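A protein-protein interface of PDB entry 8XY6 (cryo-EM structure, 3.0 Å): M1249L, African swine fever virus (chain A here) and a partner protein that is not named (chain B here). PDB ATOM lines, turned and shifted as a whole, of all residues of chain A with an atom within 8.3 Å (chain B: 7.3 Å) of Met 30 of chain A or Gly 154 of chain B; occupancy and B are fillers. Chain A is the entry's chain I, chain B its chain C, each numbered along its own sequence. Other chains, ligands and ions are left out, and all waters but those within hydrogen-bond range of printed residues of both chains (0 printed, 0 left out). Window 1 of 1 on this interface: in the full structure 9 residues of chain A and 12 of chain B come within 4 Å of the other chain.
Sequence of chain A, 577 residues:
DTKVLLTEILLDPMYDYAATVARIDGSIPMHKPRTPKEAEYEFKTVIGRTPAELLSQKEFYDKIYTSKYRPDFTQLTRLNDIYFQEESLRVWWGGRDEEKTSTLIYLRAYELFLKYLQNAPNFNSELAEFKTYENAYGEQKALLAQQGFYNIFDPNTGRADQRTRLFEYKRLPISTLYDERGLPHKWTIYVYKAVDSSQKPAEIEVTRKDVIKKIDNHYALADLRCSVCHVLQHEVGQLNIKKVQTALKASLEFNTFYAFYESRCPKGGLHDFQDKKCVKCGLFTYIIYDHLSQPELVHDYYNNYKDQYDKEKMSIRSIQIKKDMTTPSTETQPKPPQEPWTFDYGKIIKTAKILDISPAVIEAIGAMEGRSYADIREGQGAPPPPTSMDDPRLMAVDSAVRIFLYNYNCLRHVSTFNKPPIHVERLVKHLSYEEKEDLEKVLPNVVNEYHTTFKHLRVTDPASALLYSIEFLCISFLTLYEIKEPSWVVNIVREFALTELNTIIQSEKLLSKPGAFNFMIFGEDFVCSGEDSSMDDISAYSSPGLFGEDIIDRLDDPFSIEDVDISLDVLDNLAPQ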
ATOM      1  N   ALA A  19      10.311  -7.131  -1.618  1.00  0.00           N
ATOM      2  CA  ALA A  19      10.033  -6.639  -2.960  1.00  0.00           C
ATOM      3  C   ALA A  19       9.337  -7.694  -3.804  1.00  0.00           C
ATOM      4  O   ALA A  19       8.428  -7.373  -4.574  1.00  0.00           O
ATOM      5  CB  ALA A  19      11.325  -6.184  -3.633  1.00  0.00           C
ATOM      6  N   THR A  20       9.745  -8.958  -3.683  1.00  0.00           N
ATOM      7  CA  THR A  20       9.094  -9.985  -4.486  1.00  0.00           C
ATOM      8  C   THR A  20       7.688 -10.279  -3.979  1.00  0.00           C
ATOM      9  O   THR A  20       6.797 -10.585  -4.781  1.00  0.00           O
ATOM     10  CB  THR A  20       9.949 -11.253  -4.535  1.00  0.00           C
ATOM     11  OG1 THR A  20       9.583 -12.027  -5.682  1.00  0.00           O
ATOM     12  CG2 THR A  20       9.764 -12.097  -3.297  1.00  0.00           C
ATOM     13  N   VAL A  21       7.452 -10.153  -2.670  1.00  0.00           N
ATOM     14  CA  VAL A  21       6.086 -10.283  -2.171  1.00  0.00           C
ATOM     15  C   VAL A  21       5.230  -9.122  -2.663  1.00  0.00           C
ATOM     16  O   VAL A  21       4.056  -9.300  -3.006  1.00  0.00           O
ATOM     17  CB  VAL A  21       6.079 -10.396  -0.637  1.00  0.00           C
ATOM     18  CG1 VAL A  21       4.669 -10.272  -0.102  1.00  0.00           C
ATOM     19  CG2 VAL A  21       6.678 -11.721  -0.213  1.00  0.00           C
ATOM     20  N   ALA A  22       5.804  -7.918  -2.720  1.00  0.00           N
ATOM     21  CA  ALA A  22       5.081  -6.778  -3.274  1.00  0.00           C
ATOM     22  C   ALA A  22       4.767  -6.987  -4.748  1.00  0.00           C
ATOM     23  O   ALA A  22       3.671  -6.651  -5.212  1.00  0.00           O
ATOM     24  CB  ALA A  22       5.889  -5.498  -3.074  1.00  0.00           C
ATOM     25  N   ARG A  23       5.721  -7.533  -5.501  1.00  0.00           N
ATOM     26  CA  ARG A  23       5.477  -7.851  -6.903  1.00  0.00           C
ATOM     27  C   ARG A  23       4.343  -8.852  -7.045  1.00  0.00           C
ATOM     28  O   ARG A  23       3.504  -8.732  -7.945  1.00  0.00           O
ATOM     29  CB  ARG A  23       6.744  -8.407  -7.547  1.00  0.00           C
ATOM     30  CG  ARG A  23       7.622  -7.372  -8.206  1.00  0.00           C
ATOM     31  CD  ARG A  23       8.879  -8.008  -8.762  1.00  0.00           C
ATOM     32  NE  ARG A  23      10.072  -7.591  -8.038  1.00  0.00           N
ATOM     33  CZ  ARG A  23      11.009  -8.425  -7.607  1.00  0.00           C
ATOM     34  NH1 ARG A  23      10.918  -9.727  -7.808  1.00  0.00           N
ATOM     35  NH2 ARG A  23      12.062  -7.937  -6.957  1.00  0.00           N
ATOM     36  N   ILE A  24       4.307  -9.855  -6.165  1.00  0.00           N
ATOM     37  CA  ILE A  24       3.242 -10.851  -6.208  1.00  0.00           C
ATOM     38  C   ILE A  24       1.883 -10.196  -6.000  1.00  0.00           C
ATOM     39  O   ILE A  24       0.907 -10.525  -6.684  1.00  0.00           O
ATOM     40  CB  ILE A  24       3.506 -11.946  -5.164  1.00  0.00           C
ATOM     41  CG1 ILE A  24       4.638 -12.856  -5.630  1.00  0.00           C
ATOM     42  CG2 ILE A  24       2.252 -12.739  -4.908  1.00  0.00           C
ATOM     43  CD1 ILE A  24       5.043 -13.870  -4.609  1.00  0.00           C
ATOM     44  N   ASP A  25       1.799  -9.258  -5.062  1.00  0.00           N
ATOM     45  CA  ASP A  25       0.558  -8.554  -4.768  1.00  0.00           C
ATOM     46  C   ASP A  25       0.351  -7.332  -5.653  1.00  0.00           C
ATOM     47  O   ASP A  25      -0.612  -6.588  -5.447  1.00  0.00           O
ATOM     48  CB  ASP A  25       0.521  -8.152  -3.294  1.00  0.00           C
ATOM     49  CG  ASP A  25       0.845  -9.308  -2.371  1.00  0.00           C
ATOM     50  OD1 ASP A  25       0.879 -10.460  -2.854  1.00  0.00           O
ATOM     51  OD2 ASP A  25       1.063  -9.070  -1.167  1.00  0.00           O
ATOM     52  N   GLY A  26       1.234  -7.107  -6.620  1.00  0.00           N
ATOM     53  CA  GLY A  26       1.043  -6.075  -7.619  1.00  0.00           C
ATOM     54  C   GLY A  26       1.078  -4.658  -7.092  1.00  0.00           C
ATOM     55  O   GLY A  26       0.365  -3.786  -7.598  1.00  0.00           O
ATOM     56  N   SER A  27       1.910  -4.407  -6.089  1.00  0.00           N
ATOM     57  CA  SER A  27       2.116  -3.057  -5.581  1.00  0.00           C
ATOM     58  C   SER A  27       3.326  -2.378  -6.192  1.00  0.00           C
ATOM     59  O   SER A  27       3.309  -1.164  -6.396  1.00  0.00           O
ATOM     60  CB  SER A  27       2.262  -3.076  -4.055  1.00  0.00           C
ATOM     61  OG  SER A  27       1.010  -3.295  -3.433  1.00  0.00           O
ATOM     62  N   ILE A  28       4.380  -3.131  -6.488  1.00  0.00           N
ATOM     63  CA  ILE A  28       5.549  -2.586  -7.168  1.00  0.00           C
ATOM     64  C   ILE A  28       5.633  -3.225  -8.548  1.00  0.00           C
ATOM     65  O   ILE A  28       5.208  -4.376  -8.723  1.00  0.00           O
ATOM     66  CB  ILE A  28       6.829  -2.810  -6.345  1.00  0.00           C
ATOM     67  CG1 ILE A  28       7.186  -4.290  -6.254  1.00  0.00           C
ATOM     68  CG2 ILE A  28       6.660  -2.262  -4.955  1.00  0.00           C
ATOM     69  CD1 ILE A  28       8.653  -4.555  -6.483  1.00  0.00           C
ATOM     70  N   PRO A  29       6.147  -2.523  -9.555  1.00  0.00           N
ATOM     71  CA  PRO A  29       6.242  -3.122 -10.889  1.00  0.00           C
ATOM     72  C   PRO A  29       7.182  -4.315 -10.887  1.00  0.00           C
ATOM     73  O   PRO A  29       8.153  -4.369 -10.130  1.00  0.00           O
ATOM     74  CB  PRO A  29       6.789  -1.979 -11.753  1.00  0.00           C
ATOM     75  CG  PRO A  29       6.495  -0.737 -10.976  1.00  0.00           C
ATOM     76  CD  PRO A  29       6.631  -1.135  -9.544  1.00  0.00           C
ATOM     77  N   MET A  30       6.882  -5.283 -11.747  1.00  0.00           N
ATOM     78  CA  MET A  30       7.756  -6.439 -11.878  1.00  0.00           C
ATOM     79  C   MET A  30       9.017  -6.140 -12.674  1.00  0.00           C
ATOM     80  O   MET A  30       9.887  -7.012 -12.772  1.00  0.00           O
ATOM     81  CB  MET A  30       7.001  -7.618 -12.491  1.00  0.00           C
ATOM     82  CG  MET A  30       6.057  -8.265 -11.499  1.00  0.00           C
ATOM     83  SD  MET A  30       5.601  -9.954 -11.894  1.00  0.00           S
ATOM     84  CE  MET A  30       4.212 -10.146 -10.793  1.00  0.00           C
ATOM     85  N   HIS A  31       9.143  -4.945 -13.242  1.00  0.00           N
ATOM     86  CA  HIS A  31      10.460  -4.497 -13.654  1.00  0.00           C
ATOM     87  C   HIS A  31      11.312  -4.244 -12.417  1.00  0.00           C
ATOM     88  O   HIS A  31      10.807  -4.100 -11.300  1.00  0.00           O
ATOM     89  CB  HIS A  31      10.390  -3.206 -14.471  1.00  0.00           C
ATOM     90  CG  HIS A  31       9.090  -2.989 -15.175  1.00  0.00           C
ATOM     91  ND1 HIS A  31       8.715  -3.726 -16.278  1.00  0.00           N
ATOM     92  CD2 HIS A  31       8.066  -2.141 -14.923  1.00  0.00           C
ATOM     93  CE1 HIS A  31       7.521  -3.332 -16.683  1.00  0.00           C
ATOM     94  NE2 HIS A  31       7.104  -2.372 -15.877  1.00  0.00           N
ATOM     95  N   LYS A  32      12.622  -4.189 -12.624  1.00  0.00           N
ATOM     96  CA  LYS A  32      13.524  -3.738 -11.580  1.00  0.00           C
ATOM     97  C   LYS A  32      13.860  -2.288 -11.867  1.00  0.00           C
ATOM     98  O   LYS A  32      14.154  -1.964 -13.025  1.00  0.00           O
ATOM     99  CB  LYS A  32      14.784  -4.600 -11.528  1.00  0.00           C
ATOM    100  CG  LYS A  32      14.801  -5.582 -10.356  1.00  0.00           C
ATOM    101  CD  LYS A  32      13.420  -6.180 -10.126  1.00  0.00           C
ATOM    102  CE  LYS A  32      12.997  -7.085 -11.275  1.00  0.00           C
ATOM    103  NZ  LYS A  32      11.635  -7.640 -11.059  1.00  0.00           N
ATOM    104  N   PRO A  33      13.823  -1.396 -10.866  1.00  0.00           N
ATOM    105  CA  PRO A  33      13.738   0.046 -11.146  1.00  0.00           C
ATOM    106  C   PRO A  33      14.672   0.521 -12.247  1.00  0.00           C
ATOM    107  O   PRO A  33      15.898   0.523 -12.098  1.00  0.00           O
ATOM    108  CB  PRO A  33      14.107   0.684  -9.804  1.00  0.00           C
ATOM    109  CG  PRO A  33      13.826  -0.355  -8.775  1.00  0.00           C
ATOM    110  CD  PRO A  33      13.695  -1.697  -9.432  1.00  0.00           C
ATOM    111  N   ARG A  34      14.072   0.943 -13.361  1.00  0.00           N
ATOM    112  CA  ARG A  34      14.828   1.287 -14.555  1.00  0.00           C
ATOM    113  C   ARG A  34      15.531   2.630 -14.440  1.00  0.00           C
ATOM    114  O   ARG A  34      16.617   2.793 -14.999  1.00  0.00           O
ATOM    115  CB  ARG A  34      13.898   1.294 -15.769  1.00  0.00           C
ATOM    116  CG  ARG A  34      12.907   0.142 -15.798  1.00  0.00           C
ATOM    117  CD  ARG A  34      11.838   0.375 -16.848  1.00  0.00           C
ATOM    118  NE  ARG A  34      11.096  -0.840 -17.158  1.00  0.00           N
ATOM    119  CZ  ARG A  34      11.497  -1.749 -18.035  1.00  0.00           C
ATOM    120  NH1 ARG A  34      12.630  -1.610 -18.701  1.00  0.00           N
ATOM    121  NH2 ARG A  34      10.742  -2.821 -18.252  1.00  0.00           N
ATOM    122  N   GLU A  38      11.557   5.722 -10.062  1.00  0.00           N
ATOM    123  CA  GLU A  38      10.852   4.492  -9.739  1.00  0.00           C
ATOM    124  C   GLU A  38      11.561   3.712  -8.645  1.00  0.00           C
ATOM    125  O   GLU A  38      10.918   2.947  -7.916  1.00  0.00           O
ATOM    126  CB  GLU A  38      10.712   3.624 -10.991  1.00  0.00           C
ATOM    127  CG  GLU A  38       9.761   2.450 -10.857  1.00  0.00           C
ATOM    128  CD  GLU A  38      10.011   1.388 -11.907  1.00  0.00           C
ATOM    129  OE1 GLU A  38      10.674   1.701 -12.917  1.00  0.00           O
ATOM    130  OE2 GLU A  38       9.549   0.243 -11.726  1.00  0.00           O
ATOM    131  N   GLU A  42       9.905   2.032  -5.353  1.00  0.00           N
ATOM    132  CA  GLU A  42      10.107   0.671  -4.871  1.00  0.00           C
ATOM    133  C   GLU A  42      10.594   0.668  -3.430  1.00  0.00           C
ATOM    134  O   GLU A  42      10.132  -0.138  -2.616  1.00  0.00           O
ATOM    135  CB  GLU A  42      11.087  -0.074  -5.771  1.00  0.00           C
ATOM    136  CG  GLU A  42      11.291  -1.523  -5.365  1.00  0.00           C
ATOM    137  CD  GLU A  42      11.680  -2.414  -6.525  1.00  0.00           C
ATOM    138  OE1 GLU A  42      11.015  -2.345  -7.580  1.00  0.00           O
ATOM    139  OE2 GLU A  42      12.651  -3.187  -6.380  1.00  0.00           O
ATOM    140  N   TYR A 106       3.689 -19.838   1.230  1.00  0.00           N
ATOM    141  CA  TYR A 106       4.595 -18.753   0.867  1.00  0.00           C
ATOM    142  C   TYR A 106       4.290 -17.489   1.660  1.00  0.00           C
ATOM    143  O   TYR A 106       5.189 -16.877   2.255  1.00  0.00           O
ATOM    144  CB  TYR A 106       4.491 -18.480  -0.631  1.00  0.00           C
ATOM    145  CG  TYR A 106       5.530 -17.525  -1.160  1.00  0.00           C
ATOM    146  CD1 TYR A 106       5.296 -16.160  -1.190  1.00  0.00           C
ATOM    147  CD2 TYR A 106       6.746 -17.989  -1.630  1.00  0.00           C
ATOM    148  CE1 TYR A 106       6.241 -15.289  -1.670  1.00  0.00           C
ATOM    149  CE2 TYR A 106       7.695 -17.125  -2.115  1.00  0.00           C
ATOM    150  CZ  TYR A 106       7.438 -15.777  -2.132  1.00  0.00           C
ATOM    151  OH  TYR A 106       8.391 -14.913  -2.616  1.00  0.00           O
ATOM    152  N   GLU B  80      16.866  -6.808 -18.565  1.00  0.00           N
ATOM    153  CA  GLU B  80      16.193  -5.926 -17.621  1.00  0.00           C
ATOM    154  C   GLU B  80      14.825  -6.464 -17.221  1.00  0.00           C
ATOM    155  O   GLU B  80      14.493  -6.508 -16.032  1.00  0.00           O
ATOM    156  CB  GLU B  80      16.065  -4.531 -18.228  1.00  0.00           C
ATOM    157  CG  GLU B  80      15.959  -3.414 -17.211  1.00  0.00           C
ATOM    158  CD  GLU B  80      14.562  -3.275 -16.651  1.00  0.00           C
ATOM    159  OE1 GLU B  80      13.610  -3.761 -17.295  1.00  0.00           O
ATOM    160  OE2 GLU B  80      14.416  -2.682 -15.567  1.00  0.00           O
ATOM    161  N   ASP B  81      14.018  -6.878 -18.196  1.00  0.00           N
ATOM    162  CA  ASP B  81      12.646  -7.289 -17.934  1.00  0.00           C
ATOM    163  C   ASP B  81      12.520  -8.712 -17.409  1.00  0.00           C
ATOM    164  O   ASP B  81      11.494  -9.034 -16.803  1.00  0.00           O
ATOM    165  CB  ASP B  81      11.799  -7.137 -19.202  1.00  0.00           C
ATOM    166  CG  ASP B  81      12.018  -5.804 -19.892  1.00  0.00           C
ATOM    167  OD1 ASP B  81      11.608  -4.769 -19.326  1.00  0.00           O
ATOM    168  OD2 ASP B  81      12.595  -5.784 -20.997  1.00  0.00           O
ATOM    169  N   SER B  82      13.516  -9.570 -17.618  1.00  0.00           N
ATOM    170  CA  SER B  82      13.476 -10.932 -17.094  1.00  0.00           C
ATOM    171  C   SER B  82      13.959 -10.915 -15.651  1.00  0.00           C
ATOM    172  O   SER B  82      15.157 -10.774 -15.387  1.00  0.00           O
ATOM    173  CB  SER B  82      14.316 -11.884 -17.940  1.00  0.00           C
ATOM    174  OG  SER B  82      14.602 -11.332 -19.208  1.00  0.00           O
ATOM    175  N   THR B  83      13.024 -11.065 -14.721  1.00  0.00           N
ATOM    176  CA  THR B  83      13.316 -11.039 -13.298  1.00  0.00           C
ATOM    177  C   THR B  83      13.868 -12.356 -12.780  1.00  0.00           C
ATOM    178  O   THR B  83      14.698 -12.343 -11.865  1.00  0.00           O
ATOM    179  CB  THR B  83      12.049 -10.670 -12.515  1.00  0.00           C
ATOM    180  OG1 THR B  83      11.619  -9.356 -12.889  1.00  0.00           O
ATOM    181  CG2 THR B  83      12.301 -10.716 -11.020  1.00  0.00           C
ATOM    182  N   ASP B  84      13.450 -13.486 -13.346  1.00  0.00           N
ATOM    183  CA  ASP B  84      13.800 -14.781 -12.782  1.00  0.00           C
ATOM    184  C   ASP B  84      15.309 -14.958 -12.776  1.00  0.00           C
ATOM    185  O   ASP B  84      15.981 -14.688 -13.775  1.00  0.00           O
ATOM    186  CB  ASP B  84      13.140 -15.911 -13.560  1.00  0.00           C
ATOM    187  CG  ASP B  84      13.218 -17.233 -12.827  1.00  0.00           C
ATOM    188  OD1 ASP B  84      14.337 -17.737 -12.609  1.00  0.00           O
ATOM    189  OD2 ASP B  84      12.157 -17.764 -12.452  1.00  0.00           O
ATOM    190  N   SER B 114       6.034 -13.792 -19.929  1.00  0.00           N
ATOM    191  CA  SER B 114       5.406 -14.543 -18.851  1.00  0.00           C
ATOM    192  C   SER B 114       5.718 -13.865 -17.530  1.00  0.00           C
ATOM    193  O   SER B 114       6.880 -13.805 -17.124  1.00  0.00           O
ATOM    194  CB  SER B 114       5.898 -15.989 -18.836  1.00  0.00           C
ATOM    195  OG  SER B 114       7.305 -16.020 -18.732  1.00  0.00           O
ATOM    196  N   LEU B 115       4.686 -13.363 -16.867  1.00  0.00           N
ATOM    197  CA  LEU B 115       4.812 -12.729 -15.565  1.00  0.00           C
ATOM    198  C   LEU B 115       4.136 -13.611 -14.527  1.00  0.00           C
ATOM    199  O   LEU B 115       2.972 -13.987 -14.695  1.00  0.00           O
ATOM    200  CB  LEU B 115       4.179 -11.338 -15.580  1.00  0.00           C
ATOM    201  CG  LEU B 115       5.059 -10.186 -16.067  1.00  0.00           C
ATOM    202  CD1 LEU B 115       4.795  -9.882 -17.533  1.00  0.00           C
ATOM    203  CD2 LEU B 115       4.822  -8.951 -15.220  1.00  0.00           C
ATOM    204  N   ASN B 116       4.861 -13.946 -13.463  1.00  0.00           N
ATOM    205  CA  ASN B 116       4.336 -14.809 -12.404  1.00  0.00           C
ATOM    206  C   ASN B 116       3.715 -13.914 -11.336  1.00  0.00           C
ATOM    207  O   ASN B 116       4.367 -13.513 -10.374  1.00  0.00           O
ATOM    208  CB  ASN B 116       5.432 -15.699 -11.833  1.00  0.00           C
ATOM    209  CG  ASN B 116       4.887 -16.827 -10.989  1.00  0.00           C
ATOM    210  OD1 ASN B 116       3.680 -16.946 -10.797  1.00  0.00           O
ATOM    211  ND2 ASN B 116       5.773 -17.665 -10.480  1.00  0.00           N
ATOM    212  N   ASN B 117       2.431 -13.613 -11.510  1.00  0.00           N
ATOM    213  CA  ASN B 117       1.700 -12.720 -10.624  1.00  0.00           C
ATOM    214  C   ASN B 117       1.217 -13.407  -9.362  1.00  0.00           C
ATOM    215  O   ASN B 117       0.308 -12.886  -8.706  1.00  0.00           O
ATOM    216  CB  ASN B 117       0.500 -12.115 -11.358  1.00  0.00           C
ATOM    217  CG  ASN B 117       0.888 -11.420 -12.649  1.00  0.00           C
ATOM    218  OD1 ASN B 117       1.713 -10.509 -12.654  1.00  0.00           O
ATOM    219  ND2 ASN B 117       0.288 -11.845 -13.753  1.00  0.00           N
ATOM    220  N   SER B 118       1.781 -14.555  -9.002  1.00  0.00           N
ATOM    221  CA  SER B 118       1.245 -15.369  -7.923  1.00  0.00           C
ATOM    222  C   SER B 118       2.374 -15.901  -7.054  1.00  0.00           C
ATOM    223  O   SER B 118       3.554 -15.649  -7.300  1.00  0.00           O
ATOM    224  CB  SER B 118       0.414 -16.526  -8.477  1.00  0.00           C
ATOM    225  OG  SER B 118       1.034 -17.086  -9.620  1.00  0.00           O
ATOM    226  N   CYS B 119       1.992 -16.651  -6.025  1.00  0.00           N
ATOM    227  CA  CYS B 119       2.942 -17.226  -5.085  1.00  0.00           C
ATOM    228  C   CYS B 119       3.370 -18.639  -5.447  1.00  0.00           C
ATOM    229  O   CYS B 119       4.179 -19.227  -4.724  1.00  0.00           O
ATOM    230  CB  CYS B 119       2.355 -17.228  -3.672  1.00  0.00           C
ATOM    231  SG  CYS B 119       1.752 -15.629  -3.111  1.00  0.00           S
ATOM    232  N   GLU B 120       2.852 -19.205  -6.528  1.00  0.00           N
ATOM    233  CA  GLU B 120       3.252 -20.546  -6.917  1.00  0.00           C
ATOM    234  C   GLU B 120       4.337 -20.490  -7.985  1.00  0.00           C
ATOM    235  O   GLU B 120       4.478 -19.507  -8.715  1.00  0.00           O
ATOM    236  CB  GLU B 120       2.055 -21.347  -7.428  1.00  0.00           C
ATOM    237  CG  GLU B 120       1.635 -21.010  -8.847  1.00  0.00           C
ATOM    238  CD  GLU B 120       0.510 -20.000  -8.896  1.00  0.00           C
ATOM    239  OE1 GLU B 120       0.080 -19.540  -7.818  1.00  0.00           O
ATOM    240  OE2 GLU B 120       0.056 -19.665 -10.009  1.00  0.00           O
ATOM    241  N   LEU B 151       9.127 -20.512 -13.626  1.00  0.00           N
ATOM    242  CA  LEU B 151       9.342 -19.203 -13.027  1.00  0.00           C
ATOM    243  C   LEU B 151       9.104 -19.284 -11.529  1.00  0.00           C
ATOM    244  O   LEU B 151       8.125 -19.890 -11.086  1.00  0.00           O
ATOM    245  CB  LEU B 151       8.420 -18.150 -13.639  1.00  0.00           C
ATOM    246  CG  LEU B 151       8.745 -17.685 -15.053  1.00  0.00           C
ATOM    247  CD1 LEU B 151       7.684 -16.724 -15.535  1.00  0.00           C
ATOM    248  CD2 LEU B 151      10.107 -17.035 -15.090  1.00  0.00           C
ATOM    249  N   GLN B 152       9.998 -18.679 -10.756  1.00  0.00           N
ATOM    250  CA  GLN B 152       9.799 -18.579  -9.326  1.00  0.00           C
ATOM    251  C   GLN B 152       8.750 -17.509  -9.032  1.00  0.00           C
ATOM    252  O   GLN B 152       8.454 -16.674  -9.888  1.00  0.00           O
ATOM    253  CB  GLN B 152      11.122 -18.261  -8.636  1.00  0.00           C
ATOM    254  CG  GLN B 152      12.107 -19.414  -8.648  1.00  0.00           C
ATOM    255  CD  GLN B 152      11.599 -20.624  -7.891  1.00  0.00           C
ATOM    256  OE1 GLN B 152      10.828 -20.498  -6.943  1.00  0.00           O
ATOM    257  NE2 GLN B 152      12.033 -21.806  -8.306  1.00  0.00           N
ATOM    258  N   PRO B 153       8.149 -17.530  -7.841  1.00  0.00           N
ATOM    259  CA  PRO B 153       7.081 -16.567  -7.548  1.00  0.00           C
ATOM    260  C   PRO B 153       7.560 -15.130  -7.675  1.00  0.00           C
ATOM    261  O   PRO B 153       8.672 -14.786  -7.274  1.00  0.00           O
ATOM    262  CB  PRO B 153       6.695 -16.900  -6.106  1.00  0.00           C
ATOM    263  CG  PRO B 153       7.073 -18.313  -5.942  1.00  0.00           C
ATOM    264  CD  PRO B 153       8.319 -18.491  -6.741  1.00  0.00           C
ATOM    265  N   GLY B 154       6.704 -14.290  -8.249  1.00  0.00           N
ATOM    266  CA  GLY B 154       7.009 -12.888  -8.414  1.00  0.00           C
ATOM    267  C   GLY B 154       8.007 -12.568  -9.501  1.00  0.00           C
ATOM    268  O   GLY B 154       8.312 -11.389  -9.707  1.00  0.00           O
ATOM    269  N   LYS B 155       8.519 -13.568 -10.206  1.00  0.00           N
ATOM    270  CA  LYS B 155       9.533 -13.369 -11.226  1.00  0.00           C
ATOM    271  C   LYS B 155       8.908 -13.358 -12.614  1.00  0.00           C
ATOM    272  O   LYS B 155       7.848 -13.938 -12.852  1.00  0.00           O
ATOM    273  CB  LYS B 155      10.599 -14.459 -11.141  1.00  0.00           C
ATOM    274  CG  LYS B 155      11.005 -14.822  -9.726  1.00  0.00           C
ATOM    275  CD  LYS B 155      11.855 -13.741  -9.089  1.00  0.00           C
ATOM    276  CE  LYS B 155      12.198 -14.100  -7.655  1.00  0.00           C
ATOM    277  NZ  LYS B 155      13.057 -15.313  -7.584  1.00  0.00           N
ATOM    278  N   SER B 156       9.588 -12.689 -13.537  1.00  0.00           N
ATOM    279  CA  SER B 156       9.117 -12.551 -14.904  1.00  0.00           C
ATOM    280  C   SER B 156      10.238 -12.902 -15.867  1.00  0.00           C
ATOM    281  O   SER B 156      11.422 -12.795 -15.543  1.00  0.00           O
ATOM    282  CB  SER B 156       8.610 -11.132 -15.190  1.00  0.00           C
ATOM    283  OG  SER B 156       9.672 -10.197 -15.166  1.00  0.00           O
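The side-chain carboxylate of Glu 80 of chain B lies close to the backbone carbonyl oxygen of Lys 32 of chain A, at 2.7 Å.
The side-chain carboxylate (OE1) of Glu 80 of chain B lies within salt-bridge range of the guanidinium group (NH1) of Arg 34 of chain A, 2.8 Å away.
The side-chain carboxylate (OD1) of Asp 81 of chain B lies within salt-bridge range of the guanidinium group (NH1) of Arg 34 of chain A, at 3.4 Å.
OG1 of Thr 83 of chain B lies within hydrogen-bond range of O of Met 30 of chain A.
NZ of Lys 32 of chain A sits at hydrogen-bond distance from OG1 of Thr 83 of chain B (2.5 Å).
O of Pro 153 of chain B lies within hydrogen-bond range of OG1 of Thr 20 of chain A, 3.3 Å away.
O of Ile 24 of chain A sits close to O of Asn 117 of chain B (3.2 Å).
The backbone carbonyl oxygen (O) of Gly 154 of chain B sits close to the side-chain sulfur (SD) of Met 30 of chain A (3.8 Å).
The backbone NH (N) of Asp 84 of chain B is in hydrogen-bond range of the backbone carbonyl oxygen (O) of Ser 156 of chain B, 3.1 Å away.
ND2 of Asn 116 of chain B sits at hydrogen-bond distance from O of Glu 120 of chain B, 2.9 Å away.
The backbone carbonyl oxygen (O) of Gln 152 of chain B is in hydrogen-bond range of the side-chain amide nitrogen (ND2) of Asn 116 of chain B (2.9 Å).
The backbone carbonyl oxygen of Lys 155 of chain B lies within hydrogen-bond range of the backbone NH of Asn 116 of chain B (3.0 Å).
OG of Ser 118 of chain B sits at hydrogen-bond distance from OE2 of Glu 120 of chain B.
O of Met 30 of chain A sits at hydrogen-bond distance from NZ of Lys 32 of chain A (2.5 Å).
Thr 83 of chain B touches Arg 23 of chain A (CG2 to NH1, 3.6 Å).
Arg 23 of chain A touches Gly 154 of chain B.
SG of Cys 119 of chain B touches CG2 of Ile 24 of chain A, 3.4 Å away.
Ile 24 of chain A touches Pro 153 of chain B (CD1 to CB, 3.8 Å).
Ile 24 of chain A touches Gly 154 of chain B (CG1 to N, 3.6 Å).
Met 30 of chain A touches Leu 115 of chain B.
Met 30 of chain A touches Asn 116 of chain B (CE to O, 3.4 Å).
Met 30 of chain A touches Asn 117 of chain B.
OG of Ser 156 of chain B touches O of Met 30 of chain A, at 3.99 Å.
Tyr 106 of chain A touches Cys 119 of chain B (CB to CB, 3.9 Å).
Gly 154 of chain B touches just these residues of chain A: Thr 20 (3.9 Å), Arg 23 (3.6 Å), Ile 24 (3.6 Å) and Met 30 (3.8 Å).
Of the printed residues of chain B, Arg 23 of chain A touches Thr 83 and Gly 154.
Of the printed residues of chain B, Tyr 106 of chain A touches Cys 119 (3.9 Å).
His 31 of chain A touches none of the printed residues of chain B.
The nearest residue of chain A that does not touch Gly 154 of chain B is Lys 32 of chain A (5.2 Å).
The nearest printed residue of chain A that does not touch Asn 117 of chain B is Arg 23 of chain A (5.1 Å).
Hydrophobic or aromatic side chains of chain B that line the printed part of chain A: Leu 115 and Pro 153.
Of the 19 printed residues of chain A, 7 touch a printed residue of chain B.
Hydrophobic or aromatic side chains of chain A that line the printed part of chain B: Ile 24, Met 30 and Tyr 106.
Among the printed residues, 21 pairs touch across the chains.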
